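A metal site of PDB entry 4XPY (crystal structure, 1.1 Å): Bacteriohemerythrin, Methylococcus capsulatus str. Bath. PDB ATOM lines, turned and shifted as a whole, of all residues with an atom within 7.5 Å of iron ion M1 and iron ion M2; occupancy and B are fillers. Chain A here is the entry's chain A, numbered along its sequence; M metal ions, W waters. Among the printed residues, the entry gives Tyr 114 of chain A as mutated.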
ATOM      1  N   THR A  13     -33.497  13.462   8.914  1.00  0.00           N
ATOM      2  CA  THR A  13     -33.496  14.093   7.595  1.00  0.00           C
ATOM      3  C   THR A  13     -33.573  13.134   6.453  1.00  0.00           C
ATOM      4  O   THR A  13     -33.674  13.581   5.290  1.00  0.00           O
ATOM      5  CB  THR A  13     -32.250  14.950   7.412  1.00  0.00           C
ATOM      6  OG1 THR A  13     -31.104  14.090   7.379  1.00  0.00           O
ATOM      7  CG2 THR A  13     -32.071  16.047   8.445  1.00  0.00           C
ATOM      8  N   ALA A  18     -25.786  13.645   7.579  1.00  0.00           N
ATOM      9  CA  ALA A  18     -26.281  14.817   8.238  1.00  0.00           C
ATOM     10  C   ALA A  18     -26.873  14.412   9.606  1.00  0.00           C
ATOM     11  O   ALA A  18     -26.620  15.096  10.629  1.00  0.00           O
ATOM     12  CB  ALA A  18     -27.344  15.485   7.391  1.00  0.00           C
ATOM     13  N   ASP A  19     -27.612  13.333   9.646  1.00  0.00           N
ATOM     14  CA  ASP A  19     -28.088  12.862  10.938  1.00  0.00           C
ATOM     15  C   ASP A  19     -26.953  12.568  11.889  1.00  0.00           C
ATOM     16  O   ASP A  19     -27.046  12.894  13.101  1.00  0.00           O
ATOM     17  CB  ASP A  19     -28.937  11.584  10.745  1.00  0.00           C
ATOM     18  CG  ASP A  19     -30.263  11.848  10.081  1.00  0.00           C
ATOM     19  OD1 ASP A  19     -30.809  12.944  10.000  1.00  0.00           O
ATOM     20  OD2 ASP A  19     -30.820  10.753   9.605  1.00  0.00           O
ATOM     21  N   GLN A  21     -23.890  13.905  11.906  1.00  0.00           N
ATOM     22  CA  GLN A  21     -23.273  15.151  12.328  1.00  0.00           C
ATOM     23  C   GLN A  21     -24.180  15.884  13.329  1.00  0.00           C
ATOM     24  O   GLN A  21     -23.680  16.476  14.295  1.00  0.00           O
ATOM     25  CB  GLN A  21     -22.930  16.040  11.131  1.00  0.00           C
ATOM     26  CG  GLN A  21     -21.874  15.384  10.230  1.00  0.00           C
ATOM     27  CD  GLN A  21     -21.502  16.255   9.071  1.00  0.00           C
ATOM     28  OE1 GLN A  21     -22.272  17.011   8.524  1.00  0.00           O
ATOM     29  NE2 GLN A  21     -20.271  16.179   8.642  1.00  0.00           N
ATOM     30  N   HIS A  22     -25.495  15.821  13.112  1.00  0.00           N
ATOM     31  CA  HIS A  22     -26.396  16.424  14.093  1.00  0.00           C
ATOM     32  C   HIS A  22     -26.291  15.768  15.445  1.00  0.00           C
ATOM     33  O   HIS A  22     -26.287  16.440  16.487  1.00  0.00           O
ATOM     34  CB  HIS A  22     -27.839  16.352  13.590  1.00  0.00           C
ATOM     35  CG  HIS A  22     -28.074  17.202  12.361  1.00  0.00           C
ATOM     36  ND1 HIS A  22     -29.085  16.951  11.459  1.00  0.00           N
ATOM     37  CD2 HIS A  22     -27.428  18.294  11.877  1.00  0.00           C
ATOM     38  CE1 HIS A  22     -29.043  17.873  10.503  1.00  0.00           C
ATOM     39  NE2 HIS A  22     -28.051  18.694  10.713  1.00  0.00           N
ATOM     40  N   ILE A  25     -23.245  17.148  17.103  1.00  0.00           N
ATOM     41  CA  ILE A  25     -23.520  18.495  17.614  1.00  0.00           C
ATOM     42  C   ILE A  25     -24.303  18.435  18.908  1.00  0.00           C
ATOM     43  O   ILE A  25     -23.943  19.120  19.889  1.00  0.00           O
ATOM     44  CB  ILE A  25     -24.255  19.336  16.536  1.00  0.00           C
ATOM     45  CG1 ILE A  25     -23.343  19.681  15.415  1.00  0.00           C
ATOM     46  CG2 ILE A  25     -24.882  20.602  17.167  1.00  0.00           C
ATOM     47  CD1 ILE A  25     -23.971  20.238  14.196  1.00  0.00           C
ATOM     48  N   HIS A  58     -19.784  20.829   9.818  1.00  0.00           N
ATOM     49  CA  HIS A  58     -21.097  20.318   9.465  1.00  0.00           C
ATOM     50  C   HIS A  58     -21.734  21.192   8.370  1.00  0.00           C
ATOM     51  O   HIS A  58     -22.292  20.663   7.395  1.00  0.00           O
ATOM     52  CB  HIS A  58     -21.977  20.251  10.716  1.00  0.00           C
ATOM     53  CG  HIS A  58     -23.440  20.003  10.385  1.00  0.00           C
ATOM     54  ND1 HIS A  58     -23.834  18.909   9.633  1.00  0.00           N
ATOM     55  CD2 HIS A  58     -24.537  20.748  10.618  1.00  0.00           C
ATOM     56  CE1 HIS A  58     -25.152  19.009   9.466  1.00  0.00           C
ATOM     57  NE2 HIS A  58     -25.613  20.125  10.047  1.00  0.00           N
ATOM     58  N   PHE A  59     -21.702  22.474   8.566  1.00  0.00           N
ATOM     59  CA  PHE A  59     -22.337  23.356   7.577  1.00  0.00           C
ATOM     60  C   PHE A  59     -21.621  23.215   6.258  1.00  0.00           C
ATOM     61  O   PHE A  59     -22.318  23.195   5.181  1.00  0.00           O
ATOM     62  CB  PHE A  59     -22.291  24.819   8.057  1.00  0.00           C
ATOM     63  CG  PHE A  59     -23.186  25.109   9.227  1.00  0.00           C
ATOM     64  CD1 PHE A  59     -23.001  26.316   9.926  1.00  0.00           C
ATOM     65  CD2 PHE A  59     -24.223  24.262   9.654  1.00  0.00           C
ATOM     66  CE1 PHE A  59     -23.838  26.663  10.947  1.00  0.00           C
ATOM     67  CE2 PHE A  59     -25.037  24.630  10.701  1.00  0.00           C
ATOM     68  CZ  PHE A  59     -24.858  25.825  11.359  1.00  0.00           C
ATOM     69  N   GLU A  62     -22.935  19.954   4.582  1.00  0.00           N
ATOM     70  CA  GLU A  62     -24.261  20.139   3.984  1.00  0.00           C
ATOM     71  C   GLU A  62     -24.186  21.021   2.756  1.00  0.00           C
ATOM     72  O   GLU A  62     -24.831  20.710   1.717  1.00  0.00           O
ATOM     73  CB  GLU A  62     -25.236  20.844   4.952  1.00  0.00           C
ATOM     74  CG  GLU A  62     -25.722  19.959   6.096  1.00  0.00           C
ATOM     75  CD  GLU A  62     -26.854  20.639   6.872  1.00  0.00           C
ATOM     76  OE1 GLU A  62     -27.129  21.811   6.543  1.00  0.00           O
ATOM     77  OE2 GLU A  62     -27.405  19.957   7.791  1.00  0.00           O
ATOM     78  N   GLU A  63     -23.444  22.089   2.810  1.00  0.00           N
ATOM     79  CA  GLU A  63     -23.392  23.047   1.679  1.00  0.00           C
ATOM     80  C   GLU A  63     -22.770  22.429   0.461  1.00  0.00           C
ATOM     81  O   GLU A  63     -23.248  22.630  -0.683  1.00  0.00           O
ATOM     82  CB  GLU A  63     -22.615  24.294   2.096  1.00  0.00           C
ATOM     83  CG  GLU A  63     -23.356  25.124   3.108  1.00  0.00           C
ATOM     84  CD  GLU A  63     -22.609  26.153   3.830  1.00  0.00           C
ATOM     85  OE1 GLU A  63     -21.509  26.573   3.286  1.00  0.00           O
ATOM     86  OE2 GLU A  63     -23.016  26.661   4.894  1.00  0.00           O
ATOM     87  N   MET A  66     -25.476  20.097  -1.023  1.00  0.00           N
ATOM     88  CA  MET A  66     -26.569  20.875  -1.556  1.00  0.00           C
ATOM     89  C   MET A  66     -26.160  21.505  -2.870  1.00  0.00           C
ATOM     90  O   MET A  66     -26.894  21.457  -3.893  1.00  0.00           O
ATOM     91  CB  MET A  66     -27.051  21.973  -0.603  1.00  0.00           C
ATOM     92  CG  MET A  66     -27.908  21.465   0.518  1.00  0.00           C
ATOM     93  SD  MET A  66     -28.614  22.781   1.554  1.00  0.00           S
ATOM     94  CE  MET A  66     -27.191  23.356   2.493  1.00  0.00           C
ATOM     95  N   HIS A  77     -30.481  28.586   2.468  1.00  0.00           N
ATOM     96  CA  HIS A  77     -30.059  27.704   3.568  1.00  0.00           C
ATOM     97  C   HIS A  77     -28.681  28.103   4.036  1.00  0.00           C
ATOM     98  O   HIS A  77     -28.425  28.271   5.266  1.00  0.00           O
ATOM     99  CB  HIS A  77     -30.167  26.289   3.060  1.00  0.00           C
ATOM    100  CG  HIS A  77     -29.948  25.238   4.121  1.00  0.00           C
ATOM    101  ND1 HIS A  77     -30.632  24.054   4.068  1.00  0.00           N
ATOM    102  CD2 HIS A  77     -29.119  25.145   5.214  1.00  0.00           C
ATOM    103  CE1 HIS A  77     -30.207  23.298   5.102  1.00  0.00           C
ATOM    104  NE2 HIS A  77     -29.292  23.920   5.807  1.00  0.00           N
ATOM    105  N   LYS A  78     -27.766  28.294   3.127  1.00  0.00           N
ATOM    106  CA  LYS A  78     -26.416  28.737   3.482  1.00  0.00           C
ATOM    107  C   LYS A  78     -26.472  30.058   4.185  1.00  0.00           C
ATOM    108  O   LYS A  78     -25.662  30.285   5.137  1.00  0.00           O
ATOM    109  CB  LYS A  78     -25.524  28.825   2.264  1.00  0.00           C
ATOM    110  CG  LYS A  78     -24.100  29.299   2.588  1.00  0.00           C
ATOM    111  CD  LYS A  78     -23.170  29.135   1.438  1.00  0.00           C
ATOM    112  CE  LYS A  78     -21.798  29.670   1.647  1.00  0.00           C
ATOM    113  NZ  LYS A  78     -21.681  31.047   2.088  1.00  0.00           N
ATOM    114  N   GLU A  80     -28.662  31.066   6.316  1.00  0.00           N
ATOM    115  CA  GLU A  80     -28.933  30.735   7.729  1.00  0.00           C
ATOM    116  C   GLU A  80     -27.678  30.248   8.435  1.00  0.00           C
ATOM    117  O   GLU A  80     -27.371  30.713   9.564  1.00  0.00           O
ATOM    118  CB  GLU A  80     -30.053  29.663   7.855  1.00  0.00           C
ATOM    119  CG  GLU A  80     -31.355  30.008   7.138  1.00  0.00           C
ATOM    120  CD  GLU A  80     -32.003  31.312   7.522  1.00  0.00           C
ATOM    121  OE1 GLU A  80     -31.749  31.877   8.573  1.00  0.00           O
ATOM    122  OE2 GLU A  80     -32.885  31.796   6.672  1.00  0.00           O
ATOM    123  N   HIS A  81     -26.958  29.349   7.802  1.00  0.00           N
ATOM    124  CA  HIS A  81     -25.689  28.846   8.374  1.00  0.00           C
ATOM    125  C   HIS A  81     -24.730  30.012   8.633  1.00  0.00           C
ATOM    126  O   HIS A  81     -24.157  30.139   9.737  1.00  0.00           O
ATOM    127  CB  HIS A  81     -24.985  27.938   7.436  1.00  0.00           C
ATOM    128  CG  HIS A  81     -25.682  26.619   7.228  1.00  0.00           C
ATOM    129  ND1 HIS A  81     -25.199  25.710   6.301  1.00  0.00           N
ATOM    130  CD2 HIS A  81     -26.720  26.000   7.848  1.00  0.00           C
ATOM    131  CE1 HIS A  81     -25.959  24.595   6.381  1.00  0.00           C
ATOM    132  NE2 HIS A  81     -26.895  24.760   7.302  1.00  0.00           N
ATOM    133  N   TRP A 113     -31.586  27.247  18.208  1.00  0.00           N
ATOM    134  CA  TRP A 113     -31.231  27.360  16.809  1.00  0.00           C
ATOM    135  C   TRP A 113     -31.342  25.999  16.130  1.00  0.00           C
ATOM    136  O   TRP A 113     -31.956  25.879  15.039  1.00  0.00           O
ATOM    137  CB  TRP A 113     -29.840  27.967  16.666  1.00  0.00           C
ATOM    138  CG  TRP A 113     -29.542  28.400  15.276  1.00  0.00           C
ATOM    139  CD1 TRP A 113     -29.661  29.679  14.765  1.00  0.00           C
ATOM    140  CD2 TRP A 113     -29.131  27.592  14.179  1.00  0.00           C
ATOM    141  NE1 TRP A 113     -29.302  29.708  13.441  1.00  0.00           N
ATOM    142  CE2 TRP A 113     -28.980  28.429  13.050  1.00  0.00           C
ATOM    143  CE3 TRP A 113     -28.763  26.241  14.054  1.00  0.00           C
ATOM    144  CZ2 TRP A 113     -28.563  27.938  11.798  1.00  0.00           C
ATOM    145  CZ3 TRP A 113     -28.334  25.769  12.808  1.00  0.00           C
ATOM    146  CH2 TRP A 113     -28.228  26.637  11.695  1.00  0.00           C
ATOM    147  N   TYR A 114     -30.737  24.962  16.718  1.00  0.00           N
ATOM    148  CA  TYR A 114     -30.750  23.640  16.064  1.00  0.00           C
ATOM    149  C   TYR A 114     -32.102  23.011  16.031  1.00  0.00           C
ATOM    150  O   TYR A 114     -32.462  22.339  15.020  1.00  0.00           O
ATOM    151  CB  TYR A 114     -29.751  22.664  16.741  1.00  0.00           C
ATOM    152  CG  TYR A 114     -28.377  23.049  16.548  1.00  0.00           C
ATOM    153  CD1 TYR A 114     -27.807  23.057  15.358  1.00  0.00           C
ATOM    154  CD2 TYR A 114     -27.673  23.367  17.765  1.00  0.00           C
ATOM    155  CE1 TYR A 114     -26.397  23.681  15.306  1.00  0.00           C
ATOM    156  CE2 TYR A 114     -26.392  23.833  17.760  1.00  0.00           C
ATOM    157  CZ  TYR A 114     -25.886  24.098  16.544  1.00  0.00           C
ATOM    158  OH  TYR A 114     -24.572  24.534  16.528  1.00  0.00           O
ATOM    159  N   HIS A 117     -33.775  24.799  13.211  1.00  0.00           N
ATOM    160  CA  HIS A 117     -33.152  24.652  11.898  1.00  0.00           C
ATOM    161  C   HIS A 117     -33.305  23.259  11.337  1.00  0.00           C
ATOM    162  O   HIS A 117     -33.586  23.078  10.151  1.00  0.00           O
ATOM    163  CB  HIS A 117     -31.667  24.984  12.012  1.00  0.00           C
ATOM    164  CG  HIS A 117     -30.944  24.938  10.709  1.00  0.00           C
ATOM    165  ND1 HIS A 117     -30.901  26.022   9.840  1.00  0.00           N
ATOM    166  CD2 HIS A 117     -30.207  23.970  10.128  1.00  0.00           C
ATOM    167  CE1 HIS A 117     -30.145  25.684   8.802  1.00  0.00           C
ATOM    168  NE2 HIS A 117     -29.684  24.452   8.920  1.00  0.00           N
ATOM    169  N   ILE A 118     -33.099  22.219  12.168  1.00  0.00           N
ATOM    170  CA  ILE A 118     -33.065  20.893  11.615  1.00  0.00           C
ATOM    171  C   ILE A 118     -34.437  20.507  11.011  1.00  0.00           C
ATOM    172  O   ILE A 118     -34.516  20.067   9.882  1.00  0.00           O
ATOM    173  CB  ILE A 118     -32.493  19.860  12.608  1.00  0.00           C
ATOM    174  CG1 ILE A 118     -31.034  20.192  12.865  1.00  0.00           C
ATOM    175  CG2 ILE A 118     -32.678  18.440  12.021  1.00  0.00           C
ATOM    176  CD1 ILE A 118     -30.428  19.439  14.051  1.00  0.00           C
ATOM    177  N   VAL A 121     -35.498  23.514   8.124  1.00  0.00           N
ATOM    178  CA  VAL A 121     -34.562  23.872   7.101  1.00  0.00           C
ATOM    179  C   VAL A 121     -33.872  22.599   6.587  1.00  0.00           C
ATOM    180  O   VAL A 121     -33.927  22.290   5.384  1.00  0.00           O
ATOM    181  CB  VAL A 121     -33.539  24.970   7.555  1.00  0.00           C
ATOM    182  CG1 VAL A 121     -32.800  25.482   6.382  1.00  0.00           C
ATOM    183  CG2 VAL A 121     -34.300  26.103   8.251  1.00  0.00           C
ATOM    184  N   ASP A 122     -33.213  21.830   7.505  1.00  0.00           N
ATOM    185  CA  ASP A 122     -32.494  20.639   7.001  1.00  0.00           C
ATOM    186  C   ASP A 122     -33.398  19.572   6.453  1.00  0.00           C
ATOM    187  O   ASP A 122     -33.097  18.944   5.459  1.00  0.00           O
ATOM    188  CB  ASP A 122     -31.578  20.047   8.100  1.00  0.00           C
ATOM    189  CG  ASP A 122     -30.400  20.897   8.423  1.00  0.00           C
ATOM    190  OD1 ASP A 122     -30.037  21.799   7.609  1.00  0.00           O
ATOM    191  OD2 ASP A 122     -29.777  20.589   9.489  1.00  0.00           O
ATOM    192  N   LYS A 123     -34.534  19.336   7.115  1.00  0.00           N
ATOM    193  CA  LYS A 123     -35.372  18.195   6.577  1.00  0.00           C
ATOM    194  C   LYS A 123     -35.745  18.458   5.135  1.00  0.00           C
ATOM    195  O   LYS A 123     -35.994  17.488   4.383  1.00  0.00           O
ATOM    196  CB  LYS A 123     -36.626  18.018   7.401  1.00  0.00           C
ATOM    197  CG  LYS A 123     -36.430  17.318   8.718  1.00  0.00           C
ATOM    198  CD  LYS A 123     -37.729  17.003   9.416  1.00  0.00           C
ATOM    199  CE  LYS A 123     -37.558  16.356  10.740  1.00  0.00           C
ATOM    200  NZ  LYS A 123     -38.870  15.904  11.271  1.00  0.00           N
ATOM    201  N   TYR A 125     -34.000  19.246   2.608  1.00  0.00           N
ATOM    202  CA  TYR A 125     -33.097  18.762   1.648  1.00  0.00           C
ATOM    203  C   TYR A 125     -33.114  17.227   1.519  1.00  0.00           C
ATOM    204  O   TYR A 125     -32.441  16.685   0.720  1.00  0.00           O
ATOM    205  CB  TYR A 125     -31.627  19.244   1.850  1.00  0.00           C
ATOM    206  CG  TYR A 125     -30.932  18.897   3.150  1.00  0.00           C
ATOM    207  CD1 TYR A 125     -30.940  17.606   3.668  1.00  0.00           C
ATOM    208  CD2 TYR A 125     -30.245  19.898   3.797  1.00  0.00           C
ATOM    209  CE1 TYR A 125     -30.290  17.328   4.881  1.00  0.00           C
ATOM    210  CE2 TYR A 125     -29.588  19.658   4.976  1.00  0.00           C
ATOM    211  CZ  TYR A 125     -29.666  18.401   5.539  1.00  0.00           C
ATOM    212  OH  TYR A 125     -29.061  18.068   6.780  1.00  0.00           O
HETATM  213 FE    FE M   1     -27.700  20.693   9.876  1.00  0.00          FE
HETATM  214 FE    FE M   2     -28.384  23.198   7.678  1.00  0.00          FE
HETATM  215  O   HOH W   1     -27.784  21.666  12.112  1.00  0.00           O
HETATM  216  O   HOH W   2     -27.419  22.486   9.255  1.00  0.00           O
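Iron ion M2 is bound by water W2 (2.0 Å), OD1 of Asp 122 (2.2 Å), OE1 of Glu 62 (2.2 Å), NE2 of His 81 (2.2 Å), NE2 of His 117 (2.2 Å) and NE2 of His 77 (2.2 Å).
Within 4 Å of iron ion M2: Glu 62, His 77, His 81, His 117 and Asp 122. The nearest printed residue that does not touch iron ion M2 is Tyr 125 (4.6 Å).
The side-chain amide oxygen of Gln 21 sits at hydrogen-bond distance from a ring nitrogen (ND1) of His 58 (2.7 Å). OE2 of Glu 62 lies close to OH of Tyr 125 (2.7 Å). ND1 of His 81 lies within hydrogen-bond range of OE2 of Glu 63 (2.8 Å). A ring nitrogen (ND1) of His 22 sits close to the backbone carbonyl oxygen (O) of Ala 18. SD of Met 66 lies within hydrogen-bond range of ND1 of His 77 (3.5 Å).
Iron ion M1 is bound by water W2 (1.9 Å), OD2 of Asp 122 (2.1 Å), NE2 of His 58 (2.2 Å), NE2 of His 22 (2.2 Å), OE2 of Glu 62 (2.2 Å) and water W1 (2.4 Å). Iron ion M1 has six donor atoms within binding distance.
Of the 23 residues printed, 4 come within 4 Å of iron ion M1. The nearest printed residue that does not touch iron ion M1 is His 117 (4.1 Å).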
